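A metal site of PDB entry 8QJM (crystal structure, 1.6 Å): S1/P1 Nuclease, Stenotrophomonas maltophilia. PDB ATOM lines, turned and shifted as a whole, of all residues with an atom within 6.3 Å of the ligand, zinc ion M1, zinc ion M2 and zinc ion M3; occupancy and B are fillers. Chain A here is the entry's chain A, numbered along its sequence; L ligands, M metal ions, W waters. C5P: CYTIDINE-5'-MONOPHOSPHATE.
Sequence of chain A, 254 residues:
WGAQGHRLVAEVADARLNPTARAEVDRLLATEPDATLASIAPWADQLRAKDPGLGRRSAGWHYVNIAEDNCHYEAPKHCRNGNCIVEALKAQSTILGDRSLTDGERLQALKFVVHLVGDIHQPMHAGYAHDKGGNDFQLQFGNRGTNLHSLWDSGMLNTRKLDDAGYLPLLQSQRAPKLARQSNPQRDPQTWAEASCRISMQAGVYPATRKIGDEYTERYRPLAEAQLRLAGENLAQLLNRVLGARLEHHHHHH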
ATOM      1  N   TRP A   1       2.853  -0.905 -16.795  1.00  0.00           N
ATOM      2  CA  TRP A   1       3.299  -2.078 -15.945  1.00  0.00           C
ATOM      3  C   TRP A   1       2.635  -1.999 -14.574  1.00  0.00           C
ATOM      4  O   TRP A   1       2.315  -0.873 -14.114  1.00  0.00           O
ATOM      5  CB  TRP A   1       4.828  -2.087 -15.777  1.00  0.00           C
ATOM      6  CG  TRP A   1       5.551  -2.077 -17.086  1.00  0.00           C
ATOM      7  CD1 TRP A   1       6.224  -1.013 -17.619  1.00  0.00           C
ATOM      8  CD2 TRP A   1       5.668  -3.151 -18.009  1.00  0.00           C
ATOM      9  NE1 TRP A   1       6.721  -1.375 -18.839  1.00  0.00           N
ATOM     10  CE2 TRP A   1       6.384  -2.665 -19.107  1.00  0.00           C
ATOM     11  CE3 TRP A   1       5.219  -4.472 -18.057  1.00  0.00           C
ATOM     12  CZ2 TRP A   1       6.744  -3.455 -20.197  1.00  0.00           C
ATOM     13  CZ3 TRP A   1       5.516  -5.248 -19.144  1.00  0.00           C
ATOM     14  CH2 TRP A   1       6.283  -4.745 -20.202  1.00  0.00           C
ATOM     15  N   GLY A   2       2.577  -3.148 -13.887  1.00  0.00           N
ATOM     16  CA  GLY A   2       2.376  -3.264 -12.444  1.00  0.00           C
ATOM     17  C   GLY A   2       3.590  -2.718 -11.720  1.00  0.00           C
ATOM     18  O   GLY A   2       4.543  -2.241 -12.354  1.00  0.00           O
ATOM     19  N   ALA A   3       3.491  -2.664 -10.410  1.00  0.00           N
ATOM     20  CA  ALA A   3       4.489  -2.031  -9.547  1.00  0.00           C
ATOM     21  C   ALA A   3       5.843  -2.682  -9.836  1.00  0.00           C
ATOM     22  O   ALA A   3       6.841  -1.939  -9.886  1.00  0.00           O
ATOM     23  CB  ALA A   3       4.099  -2.194  -8.071  1.00  0.00           C
ATOM     24  N   HIS A   6       7.501  -1.460 -13.012  1.00  0.00           N
ATOM     25  CA  HIS A   6       8.010  -0.064 -12.867  1.00  0.00           C
ATOM     26  C   HIS A   6       9.347  -0.113 -12.138  1.00  0.00           C
ATOM     27  O   HIS A   6      10.292   0.655 -12.510  1.00  0.00           O
ATOM     28  CB  HIS A   6       6.915   0.797 -12.215  1.00  0.00           C
ATOM     29  CG  HIS A   6       5.892   1.172 -13.222  1.00  0.00           C
ATOM     30  ND1 HIS A   6       6.167   2.048 -14.258  1.00  0.00           N
ATOM     31  CD2 HIS A   6       4.611   0.751 -13.424  1.00  0.00           C
ATOM     32  CE1 HIS A   6       5.100   2.138 -15.033  1.00  0.00           C
ATOM     33  NE2 HIS A   6       4.158   1.377 -14.570  1.00  0.00           N
ATOM     34  N   ALA A  44       3.295   7.308  -9.721  1.00  0.00           N
ATOM     35  CA  ALA A  44       2.315   7.986 -10.591  1.00  0.00           C
ATOM     36  C   ALA A  44       1.001   7.183 -10.627  1.00  0.00           C
ATOM     37  O   ALA A  44      -0.031   7.855 -10.698  1.00  0.00           O
ATOM     38  CB  ALA A  44       2.915   8.242 -11.955  1.00  0.00           C
ATOM     39  N   ASP A  45       1.014   5.854 -10.499  1.00  0.00           N
ATOM     40  CA  ASP A  45      -0.239   5.033 -10.474  1.00  0.00           C
ATOM     41  C   ASP A  45      -0.959   5.234  -9.140  1.00  0.00           C
ATOM     42  O   ASP A  45      -2.210   5.236  -9.144  1.00  0.00           O
ATOM     43  CB  ASP A  45       0.031   3.547 -10.703  1.00  0.00           C
ATOM     44  CG  ASP A  45       0.538   3.226 -12.079  1.00  0.00           C
ATOM     45  OD1 ASP A  45       0.240   3.980 -13.012  1.00  0.00           O
ATOM     46  OD2 ASP A  45       1.251   2.222 -12.237  1.00  0.00           O
ATOM     47  N   GLN A  46      -0.221   5.367  -8.050  1.00  0.00           N
ATOM     48  CA  GLN A  46      -0.791   5.607  -6.707  1.00  0.00           C
ATOM     49  C   GLN A  46      -1.423   7.011  -6.706  1.00  0.00           C
ATOM     50  O   GLN A  46      -2.516   7.143  -6.186  1.00  0.00           O
ATOM     51  CB  GLN A  46       0.267   5.393  -5.627  1.00  0.00           C
ATOM     52  CG  GLN A  46       0.576   3.927  -5.402  1.00  0.00           C
ATOM     53  CD  GLN A  46      -0.684   3.090  -5.414  1.00  0.00           C
ATOM     54  OE1 GLN A  46      -1.536   3.230  -4.539  1.00  0.00           O
ATOM     55  NE2 GLN A  46      -0.815   2.218  -6.387  1.00  0.00           N
ATOM     56  N   ARG A  48      -2.672   8.565  -9.279  1.00  0.00           N
ATOM     57  CA  ARG A  48      -3.934   8.397 -10.079  1.00  0.00           C
ATOM     58  C   ARG A  48      -5.033   7.787  -9.188  1.00  0.00           C
ATOM     59  O   ARG A  48      -6.228   8.270  -9.270  1.00  0.00           O
ATOM     60  CB  ARG A  48      -3.662   7.592 -11.368  1.00  0.00           C
ATOM     61  CG  ARG A  48      -4.888   7.427 -12.260  1.00  0.00           C
ATOM     62  CD  ARG A  48      -4.665   6.440 -13.397  1.00  0.00           C
ATOM     63  NE  ARG A  48      -4.343   5.153 -12.847  1.00  0.00           N
ATOM     64  CZ  ARG A  48      -3.391   4.337 -13.291  1.00  0.00           C
ATOM     65  NH1 ARG A  48      -2.694   4.623 -14.387  1.00  0.00           N
ATOM     66  NH2 ARG A  48      -3.157   3.209 -12.643  1.00  0.00           N
ATOM     67  N   ALA A  49      -4.696   6.792  -8.374  1.00  0.00           N
ATOM     68  CA  ALA A  49      -5.660   6.073  -7.507  1.00  0.00           C
ATOM     69  C   ALA A  49      -6.174   7.002  -6.413  1.00  0.00           C
ATOM     70  O   ALA A  49      -7.396   6.935  -6.116  1.00  0.00           O
ATOM     71  CB  ALA A  49      -5.043   4.840  -6.891  1.00  0.00           C
ATOM     72  N   HIS A  62      -0.655   8.219 -18.817  1.00  0.00           N
ATOM     73  CA  HIS A  62      -0.009   6.889 -18.723  1.00  0.00           C
ATOM     74  C   HIS A  62      -0.100   6.139 -20.060  1.00  0.00           C
ATOM     75  O   HIS A  62       0.494   5.093 -20.140  1.00  0.00           O
ATOM     76  CB  HIS A  62      -0.616   6.029 -17.609  1.00  0.00           C
ATOM     77  CG  HIS A  62      -0.456   6.610 -16.252  1.00  0.00           C
ATOM     78  ND1 HIS A  62       0.219   5.951 -15.229  1.00  0.00           N
ATOM     79  CD2 HIS A  62      -0.849   7.813 -15.756  1.00  0.00           C
ATOM     80  CE1 HIS A  62       0.165   6.716 -14.155  1.00  0.00           C
ATOM     81  NE2 HIS A  62      -0.442   7.876 -14.449  1.00  0.00           N
ATOM     82  N   HIS A 115       8.362   6.736 -14.179  1.00  0.00           N
ATOM     83  CA  HIS A 115       7.105   5.989 -14.403  1.00  0.00           C
ATOM     84  C   HIS A 115       6.815   5.911 -15.896  1.00  0.00           C
ATOM     85  O   HIS A 115       6.411   4.796 -16.392  1.00  0.00           O
ATOM     86  CB  HIS A 115       5.924   6.644 -13.648  1.00  0.00           C
ATOM     87  CG  HIS A 115       4.718   5.742 -13.702  1.00  0.00           C
ATOM     88  ND1 HIS A 115       4.517   4.681 -12.819  1.00  0.00           N
ATOM     89  CD2 HIS A 115       3.706   5.710 -14.586  1.00  0.00           C
ATOM     90  CE1 HIS A 115       3.376   4.060 -13.154  1.00  0.00           C
ATOM     91  NE2 HIS A 115       2.881   4.665 -14.255  1.00  0.00           N
ATOM     92  N   LEU A 116       6.843   7.048 -16.602  1.00  0.00           N
ATOM     93  CA  LEU A 116       6.317   7.114 -17.972  1.00  0.00           C
ATOM     94  C   LEU A 116       7.237   6.441 -18.967  1.00  0.00           C
ATOM     95  O   LEU A 116       6.730   5.871 -19.932  1.00  0.00           O
ATOM     96  CB  LEU A 116       6.038   8.565 -18.337  1.00  0.00           C
ATOM     97  CG  LEU A 116       4.935   9.210 -17.522  1.00  0.00           C
ATOM     98  CD1 LEU A 116       4.786  10.689 -17.918  1.00  0.00           C
ATOM     99  CD2 LEU A 116       3.615   8.449 -17.643  1.00  0.00           C
ATOM    100  N   GLY A 118       8.755   3.745 -18.224  1.00  0.00           N
ATOM    101  CA  GLY A 118       8.152   2.405 -18.058  1.00  0.00           C
ATOM    102  C   GLY A 118       6.880   2.189 -18.877  1.00  0.00           C
ATOM    103  O   GLY A 118       6.796   1.267 -19.750  1.00  0.00           O
ATOM    104  N   ASP A 119       5.835   2.977 -18.628  1.00  0.00           N
ATOM    105  CA  ASP A 119       4.511   2.718 -19.261  1.00  0.00           C
ATOM    106  C   ASP A 119       4.621   2.778 -20.798  1.00  0.00           C
ATOM    107  O   ASP A 119       3.869   2.035 -21.460  1.00  0.00           O
ATOM    108  CB  ASP A 119       3.475   3.707 -18.724  1.00  0.00           C
ATOM    109  CG  ASP A 119       2.799   3.238 -17.451  1.00  0.00           C
ATOM    110  OD1 ASP A 119       2.998   2.062 -17.125  1.00  0.00           O
ATOM    111  OD2 ASP A 119       2.024   4.026 -16.843  1.00  0.00           O
ATOM    112  N   GLN A 122       5.275  -0.451 -22.445  1.00  0.00           N
ATOM    113  CA  GLN A 122       4.250  -1.532 -22.293  1.00  0.00           C
ATOM    114  C   GLN A 122       3.377  -1.454 -23.532  1.00  0.00           C
ATOM    115  O   GLN A 122       2.664  -0.464 -23.723  1.00  0.00           O
ATOM    116  CB  GLN A 122       3.517  -1.308 -20.976  1.00  0.00           C
ATOM    117  CG  GLN A 122       2.960  -2.594 -20.334  1.00  0.00           C
ATOM    118  CD  GLN A 122       1.813  -3.206 -21.087  1.00  0.00           C
ATOM    119  OE1 GLN A 122       1.911  -3.497 -22.279  1.00  0.00           O
ATOM    120  NE2 GLN A 122       0.703  -3.419 -20.390  1.00  0.00           N
ATOM    121  N   HIS A 125      -0.073   0.044 -23.626  1.00  0.00           N
ATOM    122  CA  HIS A 125      -0.208   1.484 -23.293  1.00  0.00           C
ATOM    123  C   HIS A 125      -0.133   2.311 -24.587  1.00  0.00           C
ATOM    124  O   HIS A 125      -0.198   3.541 -24.483  1.00  0.00           O
ATOM    125  CB  HIS A 125       0.901   1.864 -22.301  1.00  0.00           C
ATOM    126  CG  HIS A 125       0.557   1.475 -20.906  1.00  0.00           C
ATOM    127  ND1 HIS A 125       0.361   2.448 -19.939  1.00  0.00           N
ATOM    128  CD2 HIS A 125       0.319   0.291 -20.282  1.00  0.00           C
ATOM    129  CE1 HIS A 125       0.018   1.887 -18.797  1.00  0.00           C
ATOM    130  NE2 HIS A 125       0.044   0.573 -18.953  1.00  0.00           N
ATOM    131  N   ASN A 135      -7.809  -3.016 -21.686  1.00  0.00           N
ATOM    132  CA  ASN A 135      -8.469  -3.079 -20.359  1.00  0.00           C
ATOM    133  C   ASN A 135      -9.849  -3.717 -20.548  1.00  0.00           C
ATOM    134  O   ASN A 135     -10.256  -4.478 -19.667  1.00  0.00           O
ATOM    135  CB  ASN A 135      -8.529  -1.721 -19.656  1.00  0.00           C
ATOM    136  CG  ASN A 135      -7.233  -1.374 -18.955  1.00  0.00           C
ATOM    137  OD1 ASN A 135      -6.866  -2.017 -17.976  1.00  0.00           O
ATOM    138  ND2 ASN A 135      -6.547  -0.355 -19.464  1.00  0.00           N
ATOM    139  N   ASN A 147      -7.751  -9.389 -18.087  1.00  0.00           N
ATOM    140  CA  ASN A 147      -7.905  -8.616 -19.338  1.00  0.00           C
ATOM    141  C   ASN A 147      -6.519  -8.546 -19.959  1.00  0.00           C
ATOM    142  O   ASN A 147      -5.566  -8.785 -19.191  1.00  0.00           O
ATOM    143  CB  ASN A 147      -8.565  -7.266 -19.075  1.00  0.00           C
ATOM    144  CG  ASN A 147      -7.727  -6.355 -18.215  1.00  0.00           C
ATOM    145  OD1 ASN A 147      -6.722  -5.840 -18.670  1.00  0.00           O
ATOM    146  ND2 ASN A 147      -8.155  -6.143 -16.991  1.00  0.00           N
ATOM    147  N   HIS A 149      -4.749  -6.043 -21.039  1.00  0.00           N
ATOM    148  CA  HIS A 149      -3.929  -4.981 -20.388  1.00  0.00           C
ATOM    149  C   HIS A 149      -3.208  -5.519 -19.136  1.00  0.00           C
ATOM    150  O   HIS A 149      -1.951  -5.348 -19.044  1.00  0.00           O
ATOM    151  CB  HIS A 149      -4.808  -3.762 -20.040  1.00  0.00           C
ATOM    152  CG  HIS A 149      -3.959  -2.596 -19.717  1.00  0.00           C
ATOM    153  ND1 HIS A 149      -3.586  -1.676 -20.675  1.00  0.00           N
ATOM    154  CD2 HIS A 149      -3.278  -2.328 -18.586  1.00  0.00           C
ATOM    155  CE1 HIS A 149      -2.754  -0.800 -20.107  1.00  0.00           C
ATOM    156  NE2 HIS A 149      -2.533  -1.219 -18.794  1.00  0.00           N
ATOM    157  N   SER A 150      -3.949  -6.088 -18.183  1.00  0.00           N
ATOM    158  CA  SER A 150      -3.412  -6.615 -16.903  1.00  0.00           C
ATOM    159  C   SER A 150      -2.410  -7.736 -17.198  1.00  0.00           C
ATOM    160  O   SER A 150      -1.446  -7.893 -16.452  1.00  0.00           O
ATOM    161  CB  SER A 150      -4.537  -7.134 -16.018  1.00  0.00           C
ATOM    162  OG  SER A 150      -5.325  -6.039 -15.506  1.00  0.00           O
ATOM    163  N   ASP A 153       0.645  -5.826 -18.213  1.00  0.00           N
ATOM    164  CA  ASP A 153       1.145  -5.040 -17.038  1.00  0.00           C
ATOM    165  C   ASP A 153       1.833  -5.981 -16.030  1.00  0.00           C
ATOM    166  O   ASP A 153       2.897  -5.570 -15.506  1.00  0.00           O
ATOM    167  CB  ASP A 153       0.030  -4.242 -16.359  1.00  0.00           C
ATOM    168  CG  ASP A 153      -0.197  -2.827 -16.857  1.00  0.00           C
ATOM    169  OD1 ASP A 153       0.527  -2.365 -17.740  1.00  0.00           O
ATOM    170  OD2 ASP A 153      -1.108  -2.204 -16.346  1.00  0.00           O
HETATM  171  O3P C5P L   1      -1.739   0.878 -16.518  1.00  0.00           O
HETATM  172  P   C5P L   1      -0.685   1.506 -15.431  1.00  0.00           P
HETATM  173  O1P C5P L   1      -0.593   3.051 -15.509  1.00  0.00           O
HETATM  174  O2P C5P L   1       0.537   0.693 -15.621  1.00  0.00           O
HETATM  175  O5' C5P L   1      -1.289   1.196 -13.928  1.00  0.00           O
HETATM  176  C5' C5P L   1      -1.052  -0.103 -13.379  1.00  0.00           C
HETATM  177  C4' C5P L   1      -1.461  -0.064 -11.939  1.00  0.00           C
HETATM  178  O4' C5P L   1      -2.875   0.237 -11.870  1.00  0.00           O
HETATM  179  C3' C5P L   1      -1.325  -1.372 -11.165  1.00  0.00           C
HETATM  180  O3' C5P L   1      -0.023  -1.466 -10.592  1.00  0.00           O
HETATM  181  C2' C5P L   1      -2.356  -1.196 -10.040  1.00  0.00           C
HETATM  182  O2' C5P L   1      -1.896  -0.355  -8.997  1.00  0.00           O
HETATM  183  C1' C5P L   1      -3.427  -0.308 -10.683  1.00  0.00           C
HETATM  184  N1  C5P L   1      -4.657  -1.059 -11.008  1.00  0.00           N
HETATM  185  C2  C5P L   1      -5.554  -1.319  -9.963  1.00  0.00           C
HETATM  186  N3  C5P L   1      -6.668  -2.042 -10.216  1.00  0.00           N
HETATM  187  C4  C5P L   1      -6.924  -2.505 -11.445  1.00  0.00           C
HETATM  188  C5  C5P L   1      -6.028  -2.269 -12.525  1.00  0.00           C
HETATM  189  C6  C5P L   1      -4.915  -1.546 -12.272  1.00  0.00           C
HETATM  190  O2  C5P L   1      -5.316  -0.861  -8.838  1.00  0.00           O
HETATM  191  N4  C5P L   1      -8.037  -3.218 -11.628  1.00  0.00           N
HETATM  192 ZN    ZN M   1       1.078   4.131 -15.029  1.00  0.00          ZN
HETATM  193 ZN    ZN M   2       2.538   0.795 -15.485  1.00  0.00          ZN
HETATM  194 ZN    ZN M   3      -1.026  -0.490 -17.624  1.00  0.00          ZN
HETATM  195  O   HOH W   1      -2.743  -3.301 -14.378  1.00  0.00           O
HETATM  196  O   HOH W   2      -3.111   3.279 -18.053  1.00  0.00           O
HETATM  197  O   HOH W   3      -5.065  -3.406 -15.364  1.00  0.00           O
HETATM  198  O   HOH W   4       0.051  -1.466  -7.470  1.00  0.00           O
HETATM  199  O   HOH W   5       2.125   0.464 -10.411  1.00  0.00           O
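Zinc ion M2 is bound by NE2 of His 6 (1.9 Å), O2P of the ligand (2.0 Å), OD1 of Asp 119 (2.1 Å), N of Trp 1 (2.2 Å) and O of Trp 1 (2.2 Å).
CA of Gly 2 touches O3' of the ligand, 3.5 Å away.
N of Ala 3 touches O3' of the ligand, at 3.7 Å.
NE2 of Gln 46 touches O2' of the ligand (3.8 Å).
Hydrophobic or aromatic side chains that line the ligand: His 62 and His 125.
ND1 of His 62 is bound to zinc ion M1 (2.0 Å).
NE2 of His 115 is bound to zinc ion M1.
Zinc ion M1 is bound by O1P of the ligand, 2.0 Å away.
OD2 of Asp 119 binds zinc ion M1 (2.0 Å).
OD1 of Asp 45 binds zinc ion M1, at 2.2 Å.
O3P of the ligand binds zinc ion M3.
NE2 of His 125 binds zinc ion M3, at 2.0 Å.
A ring nitrogen (NE2) of His 149 binds zinc ion M3 (2.0 Å).
The side-chain carboxylate (OD2) of Asp 153 is bound to zinc ion M3, 2.1 Å away.
The side-chain carboxylate (OD1) of Asp 153 is bound to zinc ion M3, at 2.4 Å.
Zinc ion M3 has five donor atoms within binding distance.
Slightly farther from zinc ion M3 lies O2P of the ligand (2.8 Å).
O5' of the ligand is in hydrogen-bond range of NH2 of Arg 48, 3.0 Å away.
Arg 48 touches zinc ion M1.
The nearest printed residue that does not touch zinc ion M1 is His 6 (4.2 Å).
The nearest printed residue that does not touch zinc ion M2 is His 115 (4.1 Å).
Four residues have an atom within 4 Å of zinc ion M3: Trp 1, His 125, His 149 and Asp 153.
A ring nitrogen (ND1) of His 115 lies close to a ring nitrogen (ND1) of His 6, 3.4 Å away.
NH1 of Arg 48 lies close to ND1 of His 62 (3.3 Å).
The side-chain amide nitrogen (ND2) of Asn 135 lies close to a ring nitrogen (ND1) of His 149 (3.5 Å).
The side-chain amide oxygen (OD1) of Asn 147 lies within hydrogen-bond range of the backbone NH (N) of His 149 (3.1 Å).
N of Gly 2 is in hydrogen-bond range of O of Asp 153, at 2.9 Å.
The backbone NH (N) of Asp 153 lies close to the side-chain amide nitrogen (NE2) of Gln 122, 3.2 Å away.
The indole nitrogen of Trp 1 sits at hydrogen-bond distance from the backbone carbonyl oxygen of Gly 118 (2.8 Å).
The guanidinium group (NH1) of Arg 48 lies close to the side-chain carboxylate (OD1) of Asp 45 (3.3 Å).
Water W5 lies within hydrogen-bond range of the side-chain carboxylate of Asp 45 (2.7 Å), an oxygen (O3') of the ligand (2.9 Å) and the backbone NH of Ala 3 (3.4 Å).
Water W3 bridges the side-chain hydroxyl (OG) of Ser 150 (2.6 Å) and the side-chain amide oxygen (OD1) of Asn 135 (3.5 Å).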
